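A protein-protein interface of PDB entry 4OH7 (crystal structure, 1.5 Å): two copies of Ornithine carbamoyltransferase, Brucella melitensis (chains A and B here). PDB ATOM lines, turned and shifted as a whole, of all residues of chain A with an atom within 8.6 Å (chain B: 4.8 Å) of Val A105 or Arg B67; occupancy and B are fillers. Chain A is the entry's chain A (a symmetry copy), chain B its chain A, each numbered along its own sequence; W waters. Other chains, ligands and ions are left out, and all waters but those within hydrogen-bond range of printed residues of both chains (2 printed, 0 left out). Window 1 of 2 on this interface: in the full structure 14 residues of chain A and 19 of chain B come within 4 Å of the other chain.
Water W2 bridges OE2 of Glu A90 (2.7 Å) and OG1 of Thr B66 (2.9 Å).
Water W1 lies within hydrogen-bond range of the guanidinium group of Arg B67 (2.9 Å) and the side-chain hydroxyl of Tyr A109 (3.1 Å).
The side-chain hydroxyl of Thr B66 sits at hydrogen-bond distance from the backbone carbonyl oxygen of Glu A90 (2.8 Å).
O of Ala B298 sits at hydrogen-bond distance from OH of Tyr A109 (2.7 Å).
The guanidinium group of Arg B67 is in salt-bridge range of the side-chain carboxylate of Glu A97, at 3.0 Å.
NH1 of Arg B69 is in salt-bridge range of OE2 of Glu A90.
No position is printed for both chains.
Of the 18 pairs that touch across the chains among the printed residues, none has its exchanged pair printed and touching as well.
Thr B66 touches Leu A86.
Ser A96 touches Pro B275 (O to CB, 3.5 Å).
Pro B275 touches Glu A97 (CB to OE1, 3.7 Å).
Asp A101 touches Phe B295 (OD1 to CZ, 3.5 Å).
CD1 of Leu B274 touches CG2 of Val A105 (3.6 Å).
Val A105 touches Phe B295.
Val A105 touches Ala B298.
NH2 of Arg A108 touches CB of Phe B295, at 3.5 Å.
Tyr A109 touches Ser B71.
Tyr A109 touches Arg B301.
Of the printed residues of chain B, Glu A90 touches Thr B66 and Arg B69.
Of the printed residues of chain B, Ser A96 touches Pro B275 (3.5 Å).
Printed residues of chain B within 4 Å of Val A105: Arg B67 (3.9 Å), Leu B274 (3.6 Å), Phe B295 (3.8 Å) and Ala B298 (3.99 Å).
Ile A113 touches none of the printed residues of chain B.
Printed residues of chain A within 4 Å of Pro B275: Ser A96 and Glu A97.
Printed residues of chain A within 4 Å of Arg B301: Tyr A109.
O of Arg B67 sits at hydrogen-bond distance from OG of Ser B71, 2.8 Å away.
The guanidinium group of Arg B301 sits at hydrogen-bond distance from the side-chain hydroxyl of Thr B68, at 2.8 Å.
N of Asp A101 sits at hydrogen-bond distance from OG1 of Thr A98, 3.2 Å away.
OE2 of Glu A97 lies within hydrogen-bond range of OG1 of Thr A102, at 2.7 Å.
The backbone carbonyl oxygen (O) of Thr B68 sits at hydrogen-bond distance from the side-chain hydroxyl (OG) of Ser B71, at 3.3 Å.
Of the 12 printed residues of chain B, 10 touch a printed residue of chain A.
Among the printed residues, Asp or Glu carboxylates within 4 Å of a Lys or Arg side-chain nitrogen of the other chain: Glu A90 with Arg B69 (2.6 Å) and Glu A97 with Arg B67 (3.0 Å).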
ATOM      1  N   LEU A  86     -16.375  24.898  -5.241  1.00  0.00           N
ATOM      2  CA  LEU A  86     -15.499  23.817  -5.670  1.00  0.00           C
ATOM      3  C   LEU A  86     -15.740  22.572  -4.859  1.00  0.00           C
ATOM      4  O   LEU A  86     -15.743  22.592  -3.623  1.00  0.00           O
ATOM      5  CB  LEU A  86     -14.039  24.217  -5.478  1.00  0.00           C
ATOM      6  CG  LEU A  86     -13.615  25.518  -6.174  1.00  0.00           C
ATOM      7  CD1 LEU A  86     -12.326  26.104  -5.588  1.00  0.00           C
ATOM      8  CD2 LEU A  86     -13.471  25.307  -7.664  1.00  0.00           C
ATOM      9  N   GLU A  90     -13.374  18.341  -7.790  1.00  0.00           N
ATOM     10  CA  GLU A  90     -12.685  19.449  -8.472  1.00  0.00           C
ATOM     11  C   GLU A  90     -11.406  19.815  -7.751  1.00  0.00           C
ATOM     12  O   GLU A  90     -10.422  20.257  -8.361  1.00  0.00           O
ATOM     13  CB  GLU A  90     -13.572  20.677  -8.538  1.00  0.00           C
ATOM     14  CG  GLU A  90     -14.763  20.489  -9.446  1.00  0.00           C
ATOM     15  CD  GLU A  90     -15.619  21.725  -9.496  1.00  0.00           C
ATOM     16  OE1 GLU A  90     -16.240  22.030  -8.471  1.00  0.00           O
ATOM     17  OE2 GLU A  90     -15.659  22.382 -10.569  1.00  0.00           O
ATOM     18  N   MET A  91     -11.419  19.631  -6.442  1.00  0.00           N
ATOM     19  CA  MET A  91     -10.287  19.927  -5.577  1.00  0.00           C
ATOM     20  C   MET A  91     -10.280  19.011  -4.345  1.00  0.00           C
ATOM     21  O   MET A  91     -11.156  19.221  -3.477  1.00  0.00           O
ATOM     22  CB  MET A  91     -10.438  21.378  -5.092  1.00  0.00           C
ATOM     23  CG  MET A  91      -9.431  21.814  -4.050  1.00  0.00           C
ATOM     24  SD  MET A  91      -7.760  21.652  -4.678  1.00  0.00           S
ATOM     25  CE  MET A  91      -7.773  22.974  -5.896  1.00  0.00           C
ATOM     26  N   SER A  96      -3.294  16.254  -6.725  1.00  0.00           N
ATOM     27  CA  SER A  96      -2.649  16.495  -7.999  1.00  0.00           C
ATOM     28  C   SER A  96      -1.398  17.346  -7.871  1.00  0.00           C
ATOM     29  O   SER A  96      -0.649  17.470  -8.820  1.00  0.00           O
ATOM     30  CB  SER A  96      -3.644  17.169  -8.956  1.00  0.00           C
ATOM     31  OG  SER A  96      -4.725  16.284  -9.246  1.00  0.00           O
ATOM     32  N   GLU A  97      -1.176  17.908  -6.687  1.00  0.00           N
ATOM     33  CA  GLU A  97       0.005  18.750  -6.423  1.00  0.00           C
ATOM     34  C   GLU A  97       0.092  18.957  -4.917  1.00  0.00           C
ATOM     35  O   GLU A  97      -0.868  18.665  -4.203  1.00  0.00           O
ATOM     36  CB  GLU A  97      -0.129  20.130  -7.115  1.00  0.00           C
ATOM     37  CG  GLU A  97      -1.223  20.996  -6.565  1.00  0.00           C
ATOM     38  CD  GLU A  97      -1.508  22.260  -7.369  1.00  0.00           C
ATOM     39  OE1 GLU A  97      -0.707  22.628  -8.272  1.00  0.00           O
ATOM     40  OE2 GLU A  97      -2.545  22.851  -7.081  1.00  0.00           O
ATOM     41  N   THR A  98       1.203  19.478  -4.411  1.00  0.00           N
ATOM     42  CA  THR A  98       1.259  19.713  -2.960  1.00  0.00           C
ATOM     43  C   THR A  98       0.213  20.723  -2.523  1.00  0.00           C
ATOM     44  O   THR A  98      -0.231  21.600  -3.280  1.00  0.00           O
ATOM     45  CB  THR A  98       2.640  20.196  -2.515  1.00  0.00           C
ATOM     46  OG1 THR A  98       2.930  21.439  -3.164  1.00  0.00           O
ATOM     47  CG2 THR A  98       3.701  19.155  -2.845  1.00  0.00           C
ATOM     48  N   ILE A  99      -0.203  20.614  -1.271  1.00  0.00           N
ATOM     49  CA  ILE A  99      -1.127  21.595  -0.731  1.00  0.00           C
ATOM     50  C   ILE A  99      -0.517  22.983  -0.766  1.00  0.00           C
ATOM     51  O   ILE A  99      -1.226  23.961  -1.035  1.00  0.00           O
ATOM     52  CB  ILE A  99      -1.584  21.215   0.699  1.00  0.00           C
ATOM     53  CG1 ILE A  99      -2.360  19.909   0.623  1.00  0.00           C
ATOM     54  CG2 ILE A  99      -2.383  22.349   1.347  1.00  0.00           C
ATOM     55  CD1 ILE A  99      -2.904  19.443   1.968  1.00  0.00           C
ATOM     56  N   ALA A 100       0.789  23.086  -0.525  1.00  0.00           N
ATOM     57  CA  ALA A 100       1.461  24.383  -0.625  1.00  0.00           C
ATOM     58  C   ALA A 100       1.257  25.024  -1.997  1.00  0.00           C
ATOM     59  O   ALA A 100       0.923  26.221  -2.085  1.00  0.00           O
ATOM     60  CB  ALA A 100       2.943  24.257  -0.307  1.00  0.00           C
ATOM     61  N   ASP A 101       1.433  24.234  -3.057  1.00  0.00           N
ATOM     62  CA  ASP A 101       1.252  24.773  -4.407  1.00  0.00           C
ATOM     63  C   ASP A 101      -0.179  25.210  -4.648  1.00  0.00           C
ATOM     64  O   ASP A 101      -0.435  26.299  -5.203  1.00  0.00           O
ATOM     65  CB  ASP A 101       1.668  23.766  -5.483  1.00  0.00           C
ATOM     66  CG  ASP A 101       3.158  23.607  -5.608  1.00  0.00           C
ATOM     67  OD1 ASP A 101       3.940  24.368  -4.990  1.00  0.00           O
ATOM     68  OD2 ASP A 101       3.591  22.713  -6.381  1.00  0.00           O
ATOM     69  N   THR A 102      -1.147  24.417  -4.206  1.00  0.00           N
ATOM     70  CA  THR A 102      -2.546  24.808  -4.351  1.00  0.00           C
ATOM     71  C   THR A 102      -2.837  26.117  -3.622  1.00  0.00           C
ATOM     72  O   THR A 102      -3.505  27.025  -4.142  1.00  0.00           O
ATOM     73  CB  THR A 102      -3.494  23.724  -3.810  1.00  0.00           C
ATOM     74  OG1 THR A 102      -3.287  22.527  -4.544  1.00  0.00           O
ATOM     75  CG2 THR A 102      -4.950  24.183  -3.888  1.00  0.00           C
ATOM     76  N   ALA A 103      -2.372  26.209  -2.374  1.00  0.00           N
ATOM     77  CA  ALA A 103      -2.592  27.386  -1.577  1.00  0.00           C
ATOM     78  C   ALA A 103      -2.024  28.632  -2.205  1.00  0.00           C
ATOM     79  O   ALA A 103      -2.658  29.685  -2.174  1.00  0.00           O
ATOM     80  CB  ALA A 103      -1.964  27.198  -0.201  1.00  0.00           C
ATOM     81  N   LYS A 104      -0.802  28.530  -2.728  1.00  0.00           N
ATOM     82  CA  LYS A 104      -0.156  29.697  -3.284  1.00  0.00           C
ATOM     83  C   LYS A 104      -0.828  30.156  -4.571  1.00  0.00           C
ATOM     84  O   LYS A 104      -0.989  31.344  -4.774  1.00  0.00           O
ATOM     85  CB  LYS A 104       1.330  29.444  -3.462  1.00  0.00           C
ATOM     86  CG  LYS A 104       2.005  29.339  -2.108  1.00  0.00           C
ATOM     87  CD  LYS A 104       3.295  28.557  -2.156  1.00  0.00           C
ATOM     88  CE  LYS A 104       4.350  29.319  -2.940  1.00  0.00           C
ATOM     89  NZ  LYS A 104       5.689  28.683  -2.825  1.00  0.00           N
ATOM     90  N   VAL A 105      -1.274  29.217  -5.399  1.00  0.00           N
ATOM     91  CA  VAL A 105      -1.984  29.597  -6.619  1.00  0.00           C
ATOM     92  C   VAL A 105      -3.371  30.132  -6.319  1.00  0.00           C
ATOM     93  O   VAL A 105      -3.757  31.185  -6.836  1.00  0.00           O
ATOM     94  CB  VAL A 105      -2.044  28.446  -7.632  1.00  0.00           C
ATOM     95  CG1 VAL A 105      -2.943  28.797  -8.808  1.00  0.00           C
ATOM     96  CG2 VAL A 105      -0.646  28.123  -8.117  1.00  0.00           C
ATOM     97  N   LEU A 106      -4.137  29.471  -5.453  1.00  0.00           N
ATOM     98  CA  LEU A 106      -5.460  29.966  -5.178  1.00  0.00           C
ATOM     99  C   LEU A 106      -5.352  31.375  -4.553  1.00  0.00           C
ATOM    100  O   LEU A 106      -6.187  32.232  -4.826  1.00  0.00           O
ATOM    101  CB  LEU A 106      -6.219  28.949  -4.326  1.00  0.00           C
ATOM    102  CG  LEU A 106      -7.716  29.098  -4.142  1.00  0.00           C
ATOM    103  CD1 LEU A 106      -8.479  29.399  -5.421  1.00  0.00           C
ATOM    104  CD2 LEU A 106      -8.201  27.808  -3.508  1.00  0.00           C
ATOM    105  N   SER A 107      -4.315  31.622  -3.747  1.00  0.00           N
ATOM    106  CA  SER A 107      -4.063  32.963  -3.182  1.00  0.00           C
ATOM    107  C   SER A 107      -3.834  34.052  -4.208  1.00  0.00           C
ATOM    108  O   SER A 107      -4.058  35.220  -3.910  1.00  0.00           O
ATOM    109  CB  SER A 107      -2.885  32.948  -2.222  1.00  0.00           C
ATOM    110  OG  SER A 107      -3.178  32.145  -1.095  1.00  0.00           O
ATOM    111  N   ARG A 108      -3.362  33.698  -5.405  1.00  0.00           N
ATOM    112  CA  ARG A 108      -3.217  34.664  -6.486  1.00  0.00           C
ATOM    113  C   ARG A 108      -4.550  35.004  -7.168  1.00  0.00           C
ATOM    114  O   ARG A 108      -4.618  36.001  -7.894  1.00  0.00           O
ATOM    115  CB  ARG A 108      -2.286  34.118  -7.579  1.00  0.00           C
ATOM    116  CG  ARG A 108      -0.844  33.851  -7.163  1.00  0.00           C
ATOM    117  CD  ARG A 108      -0.197  35.070  -6.536  1.00  0.00           C
ATOM    118  NE  ARG A 108       1.213  34.795  -6.263  1.00  0.00           N
ATOM    119  CZ  ARG A 108       2.241  35.199  -6.998  1.00  0.00           C
ATOM    120  NH1 ARG A 108       2.103  35.948  -8.079  1.00  0.00           N
ATOM    121  NH2 ARG A 108       3.469  34.853  -6.625  1.00  0.00           N
ATOM    122  N   TYR A 109      -5.589  34.175  -6.974  1.00  0.00           N
ATOM    123  CA  TYR A 109      -6.863  34.363  -7.679  1.00  0.00           C
ATOM    124  C   TYR A 109      -7.983  34.891  -6.798  1.00  0.00           C
ATOM    125  O   TYR A 109      -8.828  35.611  -7.275  1.00  0.00           O
ATOM    126  CB  TYR A 109      -7.341  33.048  -8.295  1.00  0.00           C
ATOM    127  CG  TYR A 109      -6.441  32.434  -9.345  1.00  0.00           C
ATOM    128  CD1 TYR A 109      -5.702  33.198 -10.228  1.00  0.00           C
ATOM    129  CD2 TYR A 109      -6.367  31.038  -9.480  1.00  0.00           C
ATOM    130  CE1 TYR A 109      -4.897  32.604 -11.161  1.00  0.00           C
ATOM    131  CE2 TYR A 109      -5.572  30.432 -10.426  1.00  0.00           C
ATOM    132  CZ  TYR A 109      -4.829  31.189 -11.289  1.00  0.00           C
ATOM    133  OH  TYR A 109      -4.044  30.574 -12.231  1.00  0.00           O
ATOM    134  N   VAL A 110      -7.999  34.498  -5.528  1.00  0.00           N
ATOM    135  CA  VAL A 110      -9.115  34.809  -4.625  1.00  0.00           C
ATOM    136  C   VAL A 110      -8.624  35.535  -3.383  1.00  0.00           C
ATOM    137  O   VAL A 110      -7.405  35.695  -3.177  1.00  0.00           O
ATOM    138  CB  VAL A 110      -9.906  33.530  -4.246  1.00  0.00           C
ATOM    139  CG1 VAL A 110     -10.364  32.801  -5.513  1.00  0.00           C
ATOM    140  CG2 VAL A 110      -9.085  32.668  -3.308  1.00  0.00           C
ATOM    141  N   ILE A 113     -10.467  31.817   1.486  1.00  0.00           N
ATOM    142  CA  ILE A 113     -10.783  30.424   1.154  1.00  0.00           C
ATOM    143  C   ILE A 113     -11.540  29.826   2.320  1.00  0.00           C
ATOM    144  O   ILE A 113     -10.994  29.699   3.417  1.00  0.00           O
ATOM    145  CB  ILE A 113      -9.520  29.600   0.939  1.00  0.00           C
ATOM    146  CG1 ILE A 113      -8.646  30.212  -0.171  1.00  0.00           C
ATOM    147  CG2 ILE A 113      -9.859  28.156   0.566  1.00  0.00           C
ATOM    148  CD1 ILE A 113      -7.219  29.704  -0.151  1.00  0.00           C
ATOM    149  N   LEU A 126      -3.283  24.166   4.448  1.00  0.00           N
ATOM    150  CA  LEU A 126      -3.743  25.183   3.525  1.00  0.00           C
ATOM    151  C   LEU A 126      -3.493  26.557   4.127  1.00  0.00           C
ATOM    152  O   LEU A 126      -2.937  27.428   3.472  1.00  0.00           O
ATOM    153  CB  LEU A 126      -5.226  24.993   3.239  1.00  0.00           C
ATOM    154  CG  LEU A 126      -5.832  25.893   2.165  1.00  0.00           C
ATOM    155  CD1 LEU A 126      -5.336  25.476   0.797  1.00  0.00           C
ATOM    156  CD2 LEU A 126      -7.348  25.811   2.222  1.00  0.00           C
ATOM    157  N   TYR A 129       0.258  27.844   4.146  1.00  0.00           N
ATOM    158  CA  TYR A 129       0.828  28.319   2.906  1.00  0.00           C
ATOM    159  C   TYR A 129       0.021  29.376   2.165  1.00  0.00           C
ATOM    160  O   TYR A 129       0.564  30.011   1.269  1.00  0.00           O
ATOM    161  CB  TYR A 129       1.087  27.129   1.979  1.00  0.00           C
ATOM    162  CG  TYR A 129       2.121  26.180   2.544  1.00  0.00           C
ATOM    163  CD1 TYR A 129       3.462  26.521   2.538  1.00  0.00           C
ATOM    164  CD2 TYR A 129       1.752  24.958   3.077  1.00  0.00           C
ATOM    165  CE1 TYR A 129       4.417  25.653   3.065  1.00  0.00           C
ATOM    166  CE2 TYR A 129       2.698  24.079   3.587  1.00  0.00           C
ATOM    167  CZ  TYR A 129       4.016  24.438   3.586  1.00  0.00           C
ATOM    168  OH  TYR A 129       4.963  23.554   4.097  1.00  0.00           O
ATOM    169  N   ALA A 130      -1.251  29.563   2.523  1.00  0.00           N
ATOM    170  CA  ALA A 130      -2.057  30.588   1.869  1.00  0.00           C
ATOM    171  C   ALA A 130      -1.607  31.953   2.293  1.00  0.00           C
ATOM    172  O   ALA A 130      -1.120  32.131   3.401  1.00  0.00           O
ATOM    173  CB  ALA A 130      -3.524  30.402   2.197  1.00  0.00           C
ATOM    174  N   THR A 131      -1.768  32.937   1.418  1.00  0.00           N
ATOM    175  CA  THR A 131      -1.507  34.317   1.808  1.00  0.00           C
ATOM    176  C   THR A 131      -2.801  35.099   1.898  1.00  0.00           C
ATOM    177  O   THR A 131      -2.788  36.310   1.917  1.00  0.00           O
ATOM    178  CB  THR A 131      -0.579  35.011   0.799  1.00  0.00           C
ATOM    179  OG1 THR A 131      -1.123  34.863  -0.505  1.00  0.00           O
ATOM    180  CG2 THR A 131       0.814  34.420   0.853  1.00  0.00           C
ATOM    181  N   VAL A 132      -3.918  34.373   1.920  1.00  0.00           N
ATOM    182  CA  VAL A 132      -5.266  34.917   2.148  1.00  0.00           C
ATOM    183  C   VAL A 132      -5.860  34.121   3.292  1.00  0.00           C
ATOM    184  O   VAL A 132      -5.423  32.983   3.560  1.00  0.00           O
ATOM    185  CB  VAL A 132      -6.175  34.875   0.887  1.00  0.00           C
ATOM    186  CG1 VAL A 132      -5.554  35.681  -0.250  1.00  0.00           C
ATOM    187  CG2 VAL A 132      -6.425  33.454   0.438  1.00  0.00           C
ATOM    188  N   SER B  65     -10.566  21.087 -15.245  1.00  0.00           N
ATOM    189  CA  SER B  65      -9.372  21.943 -15.042  1.00  0.00           C
ATOM    190  C   SER B  65      -9.704  23.076 -14.104  1.00  0.00           C
ATOM    191  O   SER B  65     -10.120  24.168 -14.532  1.00  0.00           O
ATOM    192  CB  SER B  65      -8.761  22.551 -16.321  1.00  0.00           C
ATOM    193  OG  SER B  65      -7.585  23.317 -15.937  1.00  0.00           O
ATOM    194  N   THR B  66      -9.508  22.844 -12.820  1.00  0.00           N
ATOM    195  CA  THR B  66      -9.914  23.851 -11.852  1.00  0.00           C
ATOM    196  C   THR B  66      -9.141  25.164 -11.957  1.00  0.00           C
ATOM    197  O   THR B  66      -9.730  26.258 -11.839  1.00  0.00           O
ATOM    198  CB  THR B  66      -9.862  23.252 -10.443  1.00  0.00           C
ATOM    199  OG1 THR B  66     -10.777  22.134 -10.409  1.00  0.00           O
ATOM    200  CG2 THR B  66     -10.214  24.305  -9.404  1.00  0.00           C
ATOM    201  N   ARG B  67      -7.843  25.117 -12.220  1.00  0.00           N
ATOM    202  CA  ARG B  67      -7.098  26.378 -12.332  1.00  0.00           C
ATOM    203  C   ARG B  67      -7.562  27.219 -13.523  1.00  0.00           C
ATOM    204  O   ARG B  67      -7.600  28.436 -13.446  1.00  0.00           O
ATOM    205  CB  ARG B  67      -5.599  26.145 -12.365  1.00  0.00           C
ATOM    206  CG  ARG B  67      -5.128  25.437 -13.615  1.00  0.00           C
ATOM    207  CD  ARG B  67      -3.647  25.138 -13.495  1.00  0.00           C
ATOM    208  NE  ARG B  67      -3.349  24.127 -12.495  1.00  0.00           N
ATOM    209  CZ  ARG B  67      -2.740  24.325 -11.320  1.00  0.00           C
ATOM    210  NH1 ARG B  67      -2.341  25.528 -10.905  1.00  0.00           N
ATOM    211  NH2 ARG B  67      -2.531  23.288 -10.535  1.00  0.00           N
ATOM    212  N   THR B  68      -7.968  26.560 -14.601  1.00  0.00           N
ATOM    213  CA  THR B  68      -8.554  27.232 -15.772  1.00  0.00           C
ATOM    214  C   THR B  68      -9.936  27.843 -15.420  1.00  0.00           C
ATOM    215  O   THR B  68     -10.220  28.989 -15.759  1.00  0.00           O
ATOM    216  CB  THR B  68      -8.707  26.220 -16.906  1.00  0.00           C
ATOM    217  OG1 THR B  68      -7.413  25.704 -17.244  1.00  0.00           O
ATOM    218  CG2 THR B  68      -9.326  26.843 -18.111  1.00  0.00           C
ATOM    219  N   ARG B  69     -10.763  27.070 -14.722  1.00  0.00           N
ATOM    220  CA  ARG B  69     -12.059  27.562 -14.261  1.00  0.00           C
ATOM    221  C   ARG B  69     -11.887  28.783 -13.382  1.00  0.00           C
ATOM    222  O   ARG B  69     -12.543  29.803 -13.624  1.00  0.00           O
ATOM    223  CB  ARG B  69     -12.811  26.493 -13.490  1.00  0.00           C
ATOM    224  CG  ARG B  69     -14.185  26.928 -13.007  1.00  0.00           C
ATOM    225  CD  ARG B  69     -14.799  25.934 -12.060  1.00  0.00           C
ATOM    226  NE  ARG B  69     -15.913  26.553 -11.339  1.00  0.00           N
ATOM    227  CZ  ARG B  69     -16.524  26.008 -10.310  1.00  0.00           C
ATOM    228  NH1 ARG B  69     -16.192  24.800  -9.855  1.00  0.00           N
ATOM    229  NH2 ARG B  69     -17.515  26.676  -9.753  1.00  0.00           N
ATOM    230  N   VAL B  70     -11.032  28.683 -12.364  1.00  0.00           N
ATOM    231  CA  VAL B  70     -10.969  29.775 -11.399  1.00  0.00           C
ATOM    232  C   VAL B  70     -10.428  31.045 -12.053  1.00  0.00           C
ATOM    233  O   VAL B  70     -10.928  32.153 -11.816  1.00  0.00           O
ATOM    234  CB  VAL B  70     -10.159  29.371 -10.152  1.00  0.00           C
ATOM    235  CG1 VAL B  70      -9.992  30.565  -9.206  1.00  0.00           C
ATOM    236  CG2 VAL B  70     -10.869  28.254  -9.420  1.00  0.00           C
ATOM    237  N   SER B  71      -9.382  30.891 -12.849  1.00  0.00           N
ATOM    238  CA  SER B  71      -8.768  32.052 -13.489  1.00  0.00           C
ATOM    239  C   SER B  71      -9.720  32.735 -14.480  1.00  0.00           C
ATOM    240  O   SER B  71      -9.802  33.979 -14.477  1.00  0.00           O
ATOM    241  CB  SER B  71      -7.422  31.725 -14.124  1.00  0.00           C
ATOM    242  OG  SER B  71      -7.527  30.690 -15.091  1.00  0.00           O
ATOM    243  N   LEU B 274       2.032  24.488 -14.128  1.00  0.00           N
ATOM    244  CA  LEU B 274       1.369  23.721 -13.087  1.00  0.00           C
ATOM    245  C   LEU B 274       0.206  22.790 -13.427  1.00  0.00           C
ATOM    246  O   LEU B 274      -0.571  23.040 -14.343  1.00  0.00           O
ATOM    247  CB  LEU B 274       0.982  24.693 -11.960  1.00  0.00           C
ATOM    248  CG  LEU B 274       2.134  25.611 -11.532  1.00  0.00           C
ATOM    249  CD1 LEU B 274       1.683  26.543 -10.394  1.00  0.00           C
ATOM    250  CD2 LEU B 274       3.395  24.832 -11.173  1.00  0.00           C
ATOM    251  N   PRO B 275       0.063  21.699 -12.667  1.00  0.00           N
ATOM    252  CA  PRO B 275       0.843  21.301 -11.508  1.00  0.00           C
ATOM    253  C   PRO B 275       2.227  20.773 -11.852  1.00  0.00           C
ATOM    254  O   PRO B 275       2.428  20.306 -12.973  1.00  0.00           O
ATOM    255  CB  PRO B 275       0.016  20.157 -10.929  1.00  0.00           C
ATOM    256  CG  PRO B 275      -0.643  19.554 -12.146  1.00  0.00           C
ATOM    257  CD  PRO B 275      -1.007  20.741 -12.986  1.00  0.00           C
ATOM    258  N   PHE B 295       4.639  30.929  -9.975  1.00  0.00           N
ATOM    259  CA  PHE B 295       3.418  31.456  -9.326  1.00  0.00           C
ATOM    260  C   PHE B 295       2.938  32.750  -9.978  1.00  0.00           C
ATOM    261  O   PHE B 295       1.735  32.971 -10.109  1.00  0.00           O
ATOM    262  CB  PHE B 295       3.635  31.535  -7.814  1.00  0.00           C
ATOM    263  CG  PHE B 295       3.866  30.165  -7.214  1.00  0.00           C
ATOM    264  CD1 PHE B 295       2.799  29.281  -7.085  1.00  0.00           C
ATOM    265  CD2 PHE B 295       5.113  29.764  -6.801  1.00  0.00           C
ATOM    266  CE1 PHE B 295       2.996  28.007  -6.576  1.00  0.00           C
ATOM    267  CE2 PHE B 295       5.304  28.487  -6.286  1.00  0.00           C
ATOM    268  CZ  PHE B 295       4.245  27.619  -6.191  1.00  0.00           C
ATOM    269  N   ALA B 298       1.204  31.587 -13.049  1.00  0.00           N
ATOM    270  CA  ALA B 298      -0.144  31.141 -12.679  1.00  0.00           C
ATOM    271  C   ALA B 298      -1.073  32.325 -12.469  1.00  0.00           C
ATOM    272  O   ALA B 298      -2.181  32.347 -12.974  1.00  0.00           O
ATOM    273  CB  ALA B 298      -0.076  30.281 -11.426  1.00  0.00           C
ATOM    274  N   ARG B 301      -2.446  33.783 -15.661  1.00  0.00           N
ATOM    275  CA  ARG B 301      -3.614  33.225 -16.316  1.00  0.00           C
ATOM    276  C   ARG B 301      -4.810  34.151 -16.173  1.00  0.00           C
ATOM    277  O   ARG B 301      -5.539  34.371 -17.128  1.00  0.00           O
ATOM    278  CB  ARG B 301      -3.943  31.841 -15.774  1.00  0.00           C
ATOM    279  CG  ARG B 301      -2.903  30.798 -16.048  1.00  0.00           C
ATOM    280  CD  ARG B 301      -2.889  30.295 -17.480  1.00  0.00           C
ATOM    281  NE  ARG B 301      -4.084  29.532 -17.741  1.00  0.00           N
ATOM    282  CZ  ARG B 301      -4.252  28.251 -17.446  1.00  0.00           C
ATOM    283  NH1 ARG B 301      -3.300  27.552 -16.869  1.00  0.00           N
ATOM    284  NH2 ARG B 301      -5.430  27.697 -17.706  1.00  0.00           N
HETATM  285  O   HOH W   1      -2.281  28.009 -12.488  1.00  0.00           O
HETATM  286  O   HOH W   2     -13.289  22.872 -11.698  1.00  0.00           O
